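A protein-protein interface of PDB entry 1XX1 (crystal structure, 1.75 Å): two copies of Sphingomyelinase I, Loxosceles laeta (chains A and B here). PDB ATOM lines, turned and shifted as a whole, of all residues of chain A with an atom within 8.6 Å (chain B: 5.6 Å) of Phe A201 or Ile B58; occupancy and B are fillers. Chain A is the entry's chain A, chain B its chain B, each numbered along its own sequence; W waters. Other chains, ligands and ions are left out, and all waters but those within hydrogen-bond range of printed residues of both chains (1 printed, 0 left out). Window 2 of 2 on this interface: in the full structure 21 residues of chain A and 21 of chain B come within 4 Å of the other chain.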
ATOM      1  N   PRO A 168       4.202 -22.741   1.874  1.00  0.00           N
ATOM      2  CA  PRO A 168       2.765 -22.801   2.110  1.00  0.00           C
ATOM      3  C   PRO A 168       2.015 -21.933   1.113  1.00  0.00           C
ATOM      4  O   PRO A 168       2.644 -21.257   0.303  1.00  0.00           O
ATOM      5  CB  PRO A 168       2.612 -22.238   3.522  1.00  0.00           C
ATOM      6  CG  PRO A 168       3.839 -21.428   3.760  1.00  0.00           C
ATOM      7  CD  PRO A 168       4.899 -21.839   2.803  1.00  0.00           C
ATOM      8  N   TYR A 169       0.691 -21.926   1.179  1.00  0.00           N
ATOM      9  CA  TYR A 169      -0.068 -21.046   0.305  1.00  0.00           C
ATOM     10  C   TYR A 169      -0.137 -19.607   0.807  1.00  0.00           C
ATOM     11  O   TYR A 169      -0.475 -18.703   0.044  1.00  0.00           O
ATOM     12  CB  TYR A 169      -1.473 -21.601   0.059  1.00  0.00           C
ATOM     13  CG  TYR A 169      -1.404 -22.805  -0.824  1.00  0.00           C
ATOM     14  CD1 TYR A 169      -1.038 -24.033  -0.300  1.00  0.00           C
ATOM     15  CD2 TYR A 169      -1.637 -22.707  -2.203  1.00  0.00           C
ATOM     16  CE1 TYR A 169      -0.928 -25.153  -1.091  1.00  0.00           C
ATOM     17  CE2 TYR A 169      -1.527 -23.842  -3.022  1.00  0.00           C
ATOM     18  CZ  TYR A 169      -1.176 -25.059  -2.445  1.00  0.00           C
ATOM     19  OH  TYR A 169      -1.059 -26.199  -3.210  1.00  0.00           O
ATOM     20  N   LEU A 170       0.174 -19.383   2.076  1.00  0.00           N
ATOM     21  CA  LEU A 170       0.127 -18.022   2.627  1.00  0.00           C
ATOM     22  C   LEU A 170       1.513 -17.492   2.874  1.00  0.00           C
ATOM     23  O   LEU A 170       2.358 -18.247   3.335  1.00  0.00           O
ATOM     24  CB  LEU A 170      -0.546 -18.028   3.997  1.00  0.00           C
ATOM     25  CG  LEU A 170      -1.912 -18.629   4.063  1.00  0.00           C
ATOM     26  CD1 LEU A 170      -2.504 -18.239   5.408  1.00  0.00           C
ATOM     27  CD2 LEU A 170      -2.695 -18.113   2.872  1.00  0.00           C
ATOM     28  N   PRO A 171       1.747 -16.185   2.617  1.00  0.00           N
ATOM     29  CA  PRO A 171       0.870 -15.213   1.960  1.00  0.00           C
ATOM     30  C   PRO A 171       0.779 -15.442   0.457  1.00  0.00           C
ATOM     31  O   PRO A 171      -0.196 -15.033  -0.188  1.00  0.00           O
ATOM     32  CB  PRO A 171       1.557 -13.874   2.254  1.00  0.00           C
ATOM     33  CG  PRO A 171       2.995 -14.216   2.390  1.00  0.00           C
ATOM     34  CD  PRO A 171       3.009 -15.568   3.059  1.00  0.00           C
ATOM     35  N   SER A 172       1.805 -16.073  -0.107  1.00  0.00           N
ATOM     36  CA  SER A 172       1.836 -16.424  -1.522  1.00  0.00           C
ATOM     37  C   SER A 172       2.533 -17.765  -1.624  1.00  0.00           C
ATOM     38  O   SER A 172       3.233 -18.186  -0.698  1.00  0.00           O
ATOM     39  CB  SER A 172       2.615 -15.379  -2.359  1.00  0.00           C
ATOM     40  OG  SER A 172       2.484 -14.046  -1.851  1.00  0.00           O
ATOM     41  N   LEU A 173       2.329 -18.443  -2.742  1.00  0.00           N
ATOM     42  CA  LEU A 173       3.087 -19.646  -3.055  1.00  0.00           C
ATOM     43  C   LEU A 173       4.549 -19.315  -3.321  1.00  0.00           C
ATOM     44  O   LEU A 173       4.852 -18.292  -3.933  1.00  0.00           O
ATOM     45  CB  LEU A 173       2.465 -20.363  -4.236  1.00  0.00           C
ATOM     46  CG  LEU A 173       1.267 -21.207  -3.792  1.00  0.00           C
ATOM     47  CD1 LEU A 173       0.597 -21.791  -4.981  1.00  0.00           C
ATOM     48  CD2 LEU A 173       1.762 -22.315  -2.871  1.00  0.00           C
ATOM     49  N   PRO A 174       5.474 -20.162  -2.835  1.00  0.00           N
ATOM     50  CA  PRO A 174       6.872 -19.818  -3.050  1.00  0.00           C
ATOM     51  C   PRO A 174       7.235 -19.931  -4.506  1.00  0.00           C
ATOM     52  O   PRO A 174       6.620 -20.702  -5.264  1.00  0.00           O
ATOM     53  CB  PRO A 174       7.629 -20.846  -2.212  1.00  0.00           C
ATOM     54  CG  PRO A 174       6.694 -22.008  -2.137  1.00  0.00           C
ATOM     55  CD  PRO A 174       5.316 -21.437  -2.113  1.00  0.00           C
ATOM     56  N   ASP A 196       1.882 -29.934  -8.710  1.00  0.00           N
ATOM     57  CA  ASP A 196       1.114 -28.758  -9.064  1.00  0.00           C
ATOM     58  C   ASP A 196      -0.367 -29.106  -9.135  1.00  0.00           C
ATOM     59  O   ASP A 196      -0.743 -30.270  -9.329  1.00  0.00           O
ATOM     60  CB  ASP A 196       1.590 -28.191 -10.400  1.00  0.00           C
ATOM     61  CG  ASP A 196       1.452 -26.674 -10.476  1.00  0.00           C
ATOM     62  OD1 ASP A 196       0.490 -26.124  -9.890  1.00  0.00           O
ATOM     63  OD2 ASP A 196       2.333 -26.033 -11.094  1.00  0.00           O
ATOM     64  N   GLY A 197      -1.195 -28.079  -8.963  1.00  0.00           N
ATOM     65  CA  GLY A 197      -2.632 -28.200  -9.118  1.00  0.00           C
ATOM     66  C   GLY A 197      -3.468 -28.359  -7.856  1.00  0.00           C
ATOM     67  O   GLY A 197      -4.672 -28.575  -7.970  1.00  0.00           O
ATOM     68  N   LEU A 198      -2.860 -28.279  -6.666  1.00  0.00           N
ATOM     69  CA  LEU A 198      -3.636 -28.345  -5.405  1.00  0.00           C
ATOM     70  C   LEU A 198      -4.701 -27.248  -5.396  1.00  0.00           C
ATOM     71  O   LEU A 198      -5.871 -27.508  -5.085  1.00  0.00           O
ATOM     72  CB  LEU A 198      -2.754 -28.204  -4.153  1.00  0.00           C
ATOM     73  CG  LEU A 198      -3.150 -28.915  -2.824  1.00  0.00           C
ATOM     74  CD1 LEU A 198      -2.520 -28.297  -1.553  1.00  0.00           C
ATOM     75  CD2 LEU A 198      -4.649 -29.168  -2.587  1.00  0.00           C
ATOM     76  N   THR A 199      -4.283 -26.029  -5.744  1.00  0.00           N
ATOM     77  CA  THR A 199      -5.206 -24.914  -5.952  1.00  0.00           C
ATOM     78  C   THR A 199      -5.231 -24.500  -7.420  1.00  0.00           C
ATOM     79  O   THR A 199      -4.283 -24.772  -8.170  1.00  0.00           O
ATOM     80  CB  THR A 199      -4.807 -23.653  -5.128  1.00  0.00           C
ATOM     81  OG1 THR A 199      -3.475 -23.245  -5.473  1.00  0.00           O
ATOM     82  CG2 THR A 199      -4.880 -23.916  -3.639  1.00  0.00           C
ATOM     83  N   ASN A 200      -6.341 -23.884  -7.826  1.00  0.00           N
ATOM     84  CA  ASN A 200      -6.373 -23.013  -9.005  1.00  0.00           C
ATOM     85  C   ASN A 200      -7.025 -21.667  -8.650  1.00  0.00           C
ATOM     86  O   ASN A 200      -8.027 -21.245  -9.248  1.00  0.00           O
ATOM     87  CB  ASN A 200      -6.953 -23.693 -10.270  1.00  0.00           C
ATOM     88  CG  ASN A 200      -8.293 -24.385 -10.034  1.00  0.00           C
ATOM     89  OD1 ASN A 200      -8.692 -24.661  -8.899  1.00  0.00           O
ATOM     90  ND2 ASN A 200      -8.989 -24.683 -11.128  1.00  0.00           N
ATOM     91  N   PHE A 201      -6.419 -21.023  -7.647  1.00  0.00           N
ATOM     92  CA  PHE A 201      -6.831 -19.713  -7.122  1.00  0.00           C
ATOM     93  C   PHE A 201      -6.428 -18.547  -8.030  1.00  0.00           C
ATOM     94  O   PHE A 201      -6.767 -17.392  -7.753  1.00  0.00           O
ATOM     95  CB  PHE A 201      -6.201 -19.493  -5.754  1.00  0.00           C
ATOM     96  CG  PHE A 201      -4.720 -19.198  -5.807  1.00  0.00           C
ATOM     97  CD1 PHE A 201      -3.794 -20.230  -5.997  1.00  0.00           C
ATOM     98  CD2 PHE A 201      -4.250 -17.889  -5.656  1.00  0.00           C
ATOM     99  CE1 PHE A 201      -2.425 -19.970  -6.031  1.00  0.00           C
ATOM    100  CE2 PHE A 201      -2.878 -17.613  -5.692  1.00  0.00           C
ATOM    101  CZ  PHE A 201      -1.964 -18.660  -5.878  1.00  0.00           C
ATOM    102  N   SER A 202      -5.663 -18.856  -9.074  1.00  0.00           N
ATOM    103  CA  SER A 202      -5.307 -17.903 -10.118  1.00  0.00           C
ATOM    104  C   SER A 202      -4.991 -18.701 -11.380  1.00  0.00           C
ATOM    105  O   SER A 202      -3.824 -19.009 -11.635  1.00  0.00           O
ATOM    106  CB  SER A 202      -4.113 -17.033  -9.694  1.00  0.00           C
ATOM    107  OG  SER A 202      -3.549 -16.353 -10.810  1.00  0.00           O
ATOM    108  N   PRO A 203      -6.031 -19.036 -12.176  1.00  0.00           N
ATOM    109  CA  PRO A 203      -5.902 -19.955 -13.316  1.00  0.00           C
ATOM    110  C   PRO A 203      -4.762 -19.587 -14.272  1.00  0.00           C
ATOM    111  O   PRO A 203      -4.020 -20.467 -14.718  1.00  0.00           O
ATOM    112  CB  PRO A 203      -7.260 -19.826 -14.023  1.00  0.00           C
ATOM    113  CG  PRO A 203      -8.201 -19.453 -12.935  1.00  0.00           C
ATOM    114  CD  PRO A 203      -7.413 -18.533 -12.044  1.00  0.00           C
ATOM    115  N   LEU A 204      -4.631 -18.292 -14.557  1.00  0.00           N
ATOM    116  CA  LEU A 204      -3.597 -17.765 -15.452  1.00  0.00           C
ATOM    117  C   LEU A 204      -2.193 -18.036 -14.893  1.00  0.00           C
ATOM    118  O   LEU A 204      -1.361 -18.663 -15.558  1.00  0.00           O
ATOM    119  CB  LEU A 204      -3.818 -16.258 -15.686  1.00  0.00           C
ATOM    120  CG  LEU A 204      -5.270 -15.801 -15.940  1.00  0.00           C
ATOM    121  CD1 LEU A 204      -5.502 -14.329 -15.553  1.00  0.00           C
ATOM    122  CD2 LEU A 204      -5.710 -16.071 -17.386  1.00  0.00           C
ATOM    123  N   GLY A 205      -1.953 -17.573 -13.664  1.00  0.00           N
ATOM    124  CA  GLY A 205      -0.690 -17.792 -12.955  1.00  0.00           C
ATOM    125  C   GLY A 205      -0.423 -19.260 -12.652  1.00  0.00           C
ATOM    126  O   GLY A 205       0.728 -19.687 -12.576  1.00  0.00           O
ATOM    127  N   ASP A 206      -1.498 -20.024 -12.474  1.00  0.00           N
ATOM    128  CA  ASP A 206      -1.428 -21.481 -12.348  1.00  0.00           C
ATOM    129  C   ASP A 206      -0.904 -22.141 -13.623  1.00  0.00           C
ATOM    130  O   ASP A 206      -0.018 -23.000 -13.553  1.00  0.00           O
ATOM    131  CB  ASP A 206      -2.800 -22.056 -11.991  1.00  0.00           C
ATOM    132  CG  ASP A 206      -3.105 -21.965 -10.506  1.00  0.00           C
ATOM    133  OD1 ASP A 206      -2.651 -21.012  -9.829  1.00  0.00           O
ATOM    134  OD2 ASP A 206      -3.810 -22.862 -10.013  1.00  0.00           O
ATOM    135  N   ARG A 209       2.705 -21.183 -13.955  1.00  0.00           N
ATOM    136  CA  ARG A 209       3.506 -21.873 -12.948  1.00  0.00           C
ATOM    137  C   ARG A 209       3.859 -23.304 -13.384  1.00  0.00           C
ATOM    138  O   ARG A 209       4.995 -23.737 -13.220  1.00  0.00           O
ATOM    139  CB  ARG A 209       2.800 -21.853 -11.587  1.00  0.00           C
ATOM    140  CG  ARG A 209       3.500 -22.627 -10.504  1.00  0.00           C
ATOM    141  CD  ARG A 209       3.439 -21.940  -9.152  1.00  0.00           C
ATOM    142  NE  ARG A 209       4.571 -22.370  -8.331  1.00  0.00           N
ATOM    143  CZ  ARG A 209       5.657 -21.636  -8.082  1.00  0.00           C
ATOM    144  NH1 ARG A 209       5.765 -20.396  -8.558  1.00  0.00           N
ATOM    145  NH2 ARG A 209       6.636 -22.145  -7.339  1.00  0.00           N
ATOM    146  N   TYR B  46      -7.840 -19.204   7.907  1.00  0.00           N
ATOM    147  CA  TYR B  46      -7.436 -19.775   6.651  1.00  0.00           C
ATOM    148  C   TYR B  46      -7.923 -21.202   6.623  1.00  0.00           C
ATOM    149  O   TYR B  46      -7.762 -21.916   7.588  1.00  0.00           O
ATOM    150  CB  TYR B  46      -5.923 -19.805   6.597  1.00  0.00           C
ATOM    151  CG  TYR B  46      -5.362 -20.614   5.444  1.00  0.00           C
ATOM    152  CD1 TYR B  46      -5.381 -20.115   4.128  1.00  0.00           C
ATOM    153  CD2 TYR B  46      -4.802 -21.849   5.672  1.00  0.00           C
ATOM    154  CE1 TYR B  46      -4.834 -20.857   3.081  1.00  0.00           C
ATOM    155  CE2 TYR B  46      -4.282 -22.600   4.632  1.00  0.00           C
ATOM    156  CZ  TYR B  46      -4.287 -22.084   3.354  1.00  0.00           C
ATOM    157  OH  TYR B  46      -3.748 -22.837   2.329  1.00  0.00           O
ATOM    158  N   GLY B  48      -7.649 -23.328   3.374  1.00  0.00           N
ATOM    159  CA  GLY B  48      -6.798 -24.125   2.495  1.00  0.00           C
ATOM    160  C   GLY B  48      -7.571 -25.069   1.601  1.00  0.00           C
ATOM    161  O   GLY B  48      -8.768 -25.269   1.756  1.00  0.00           O
ATOM    162  N   THR B  49      -6.860 -25.688   0.669  1.00  0.00           N
ATOM    163  CA  THR B  49      -7.486 -26.611  -0.255  1.00  0.00           C
ATOM    164  C   THR B  49      -7.407 -28.024   0.320  1.00  0.00           C
ATOM    165  O   THR B  49      -6.446 -28.368   1.014  1.00  0.00           O
ATOM    166  CB  THR B  49      -6.773 -26.604  -1.612  1.00  0.00           C
ATOM    167  OG1 THR B  49      -5.365 -26.698  -1.383  1.00  0.00           O
ATOM    168  CG2 THR B  49      -7.063 -25.312  -2.346  1.00  0.00           C
ATOM    169  N   ASP B  56     -13.072 -20.189  -3.483  1.00  0.00           N
ATOM    170  CA  ASP B  56     -11.647 -20.068  -3.403  1.00  0.00           C
ATOM    171  C   ASP B  56     -11.286 -20.436  -1.959  1.00  0.00           C
ATOM    172  O   ASP B  56     -11.961 -20.035  -1.004  1.00  0.00           O
ATOM    173  CB  ASP B  56     -11.226 -18.639  -3.761  1.00  0.00           C
ATOM    174  CG  ASP B  56     -11.327 -18.360  -5.279  1.00  0.00           C
ATOM    175  OD1 ASP B  56     -11.278 -19.315  -6.088  1.00  0.00           O
ATOM    176  OD2 ASP B  56     -11.447 -17.182  -5.650  1.00  0.00           O
ATOM    177  N   CYS B  57     -10.276 -21.266  -1.823  1.00  0.00           N
ATOM    178  CA  CYS B  57      -9.993 -21.923  -0.545  1.00  0.00           C
ATOM    179  C   CYS B  57      -8.936 -21.228   0.295  1.00  0.00           C
ATOM    180  O   CYS B  57      -8.725 -21.605   1.427  1.00  0.00           O
ATOM    181  CB  CYS B  57      -9.479 -23.334  -0.802  1.00  0.00           C
ATOM    182  SG  CYS B  57     -10.508 -24.300  -1.879  1.00  0.00           S
ATOM    183  N   ILE B  58      -8.235 -20.259  -0.277  1.00  0.00           N
ATOM    184  CA  ILE B  58      -6.986 -19.835   0.352  1.00  0.00           C
ATOM    185  C   ILE B  58      -6.978 -18.381   0.804  1.00  0.00           C
ATOM    186  O   ILE B  58      -5.906 -17.813   1.021  1.00  0.00           O
ATOM    187  CB  ILE B  58      -5.731 -20.166  -0.503  1.00  0.00           C
ATOM    188  CG1 ILE B  58      -5.834 -19.521  -1.871  1.00  0.00           C
ATOM    189  CG2 ILE B  58      -5.550 -21.674  -0.571  1.00  0.00           C
ATOM    190  CD1 ILE B  58      -4.475 -19.402  -2.576  1.00  0.00           C
ATOM    191  N   ARG B  59      -8.176 -17.807   0.938  1.00  0.00           N
ATOM    192  CA  ARG B  59      -8.335 -16.455   1.497  1.00  0.00           C
ATOM    193  C   ARG B  59      -7.933 -16.545   2.964  1.00  0.00           C
ATOM    194  O   ARG B  59      -8.106 -17.573   3.606  1.00  0.00           O
ATOM    195  CB  ARG B  59      -9.784 -15.974   1.354  1.00  0.00           C
ATOM    196  CG  ARG B  59     -10.246 -15.835  -0.095  1.00  0.00           C
ATOM    197  CD  ARG B  59      -9.409 -14.805  -0.856  1.00  0.00           C
ATOM    198  NE  ARG B  59      -9.712 -13.435  -0.430  1.00  0.00           N
ATOM    199  CZ  ARG B  59     -10.831 -12.766  -0.726  1.00  0.00           C
ATOM    200  NH1 ARG B  59     -11.806 -13.319  -1.457  1.00  0.00           N
ATOM    201  NH2 ARG B  59     -10.991 -11.532  -0.267  1.00  0.00           N
ATOM    202  N   TRP B  60      -7.330 -15.487   3.496  1.00  0.00           N
ATOM    203  CA  TRP B  60      -6.815 -15.612   4.834  1.00  0.00           C
ATOM    204  C   TRP B  60      -6.640 -14.275   5.481  1.00  0.00           C
ATOM    205  O   TRP B  60      -6.715 -13.246   4.827  1.00  0.00           O
ATOM    206  CB  TRP B  60      -5.458 -16.335   4.820  1.00  0.00           C
ATOM    207  CG  TRP B  60      -4.406 -15.505   4.172  1.00  0.00           C
ATOM    208  CD1 TRP B  60      -4.203 -15.335   2.828  1.00  0.00           C
ATOM    209  CD2 TRP B  60      -3.394 -14.736   4.831  1.00  0.00           C
ATOM    210  NE1 TRP B  60      -3.132 -14.495   2.616  1.00  0.00           N
ATOM    211  CE2 TRP B  60      -2.618 -14.118   3.823  1.00  0.00           C
ATOM    212  CE3 TRP B  60      -3.071 -14.497   6.168  1.00  0.00           C
ATOM    213  CZ2 TRP B  60      -1.536 -13.284   4.120  1.00  0.00           C
ATOM    214  CZ3 TRP B  60      -1.993 -13.658   6.460  1.00  0.00           C
ATOM    215  CH2 TRP B  60      -1.251 -13.060   5.434  1.00  0.00           C
HETATM  216  O   HOH W   1      -0.432 -23.517   3.210  1.00  0.00           O
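O of Thr A199 sits close to OD2 of Asp A206.
CB of Tyr A169 touches OH of Tyr B46 (3.4 Å).
Leu A170 touches Tyr B46 (CD2 to CE1, 3.5 Å).
Ile B58 touches Leu A170.
Trp B60 touches Leu A170 (CD1 to CD2, 3.2 Å).
CB of Pro A171 touches CZ2 of Trp B60, at 3.7 Å.
Thr B49 touches Leu A198.
Thr B49 touches Thr A199 (CG2 to CG2, 2.9 Å).
Thr A199 touches Ile B58.
Ile B58 touches Phe A201.
Printed residues of chain B within 4 Å of Phe A201: Ile B58.
Ile B58 touches three residues of chain A.
Printed residues of chain A within 4 Å of Tyr B46: Tyr A169 (3.4 Å) and Leu A170 (3.5 Å).
Of the printed residues of chain A, Trp B60 touches Leu A170 and Pro A171.
Of the printed residues of chain B, Pro A171 touches Trp B60.
Arg B59 touches none of the printed residues of chain A.
Leu A204 touches none of the printed residues of chain B.
The nearest residue of chain A that does not touch Ile B58 is Tyr A169 (4.1 Å).
The nearest printed residue of chain B that does not touch Leu A170 is Arg B59 (5.5 Å).
Hydrophobic or aromatic side chains of chain A within 4 Å of the printed part of chain B: Tyr A169, Leu A170, Pro A171, Leu A198 and Phe A201.
Printed residues of chain B that touch a printed residue of chain A: Tyr B46, Thr B49, Ile B58 and Trp B60.
Among the printed residues, 9 pairs touch across the chains.
Among the printed residues, no Asp or Glu carboxylate lies within 4 Å of a Lys or Arg side-chain nitrogen of the other chain.
No position is printed for both chains.
Of the 9 pairs that touch across the chains among the printed residues, none has its exchanged pair printed and touching as well.
Water W1 bridges the backbone NH of Tyr A169 (2.8 Å) and the side-chain hydroxyl of Tyr B46 (3.5 Å).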
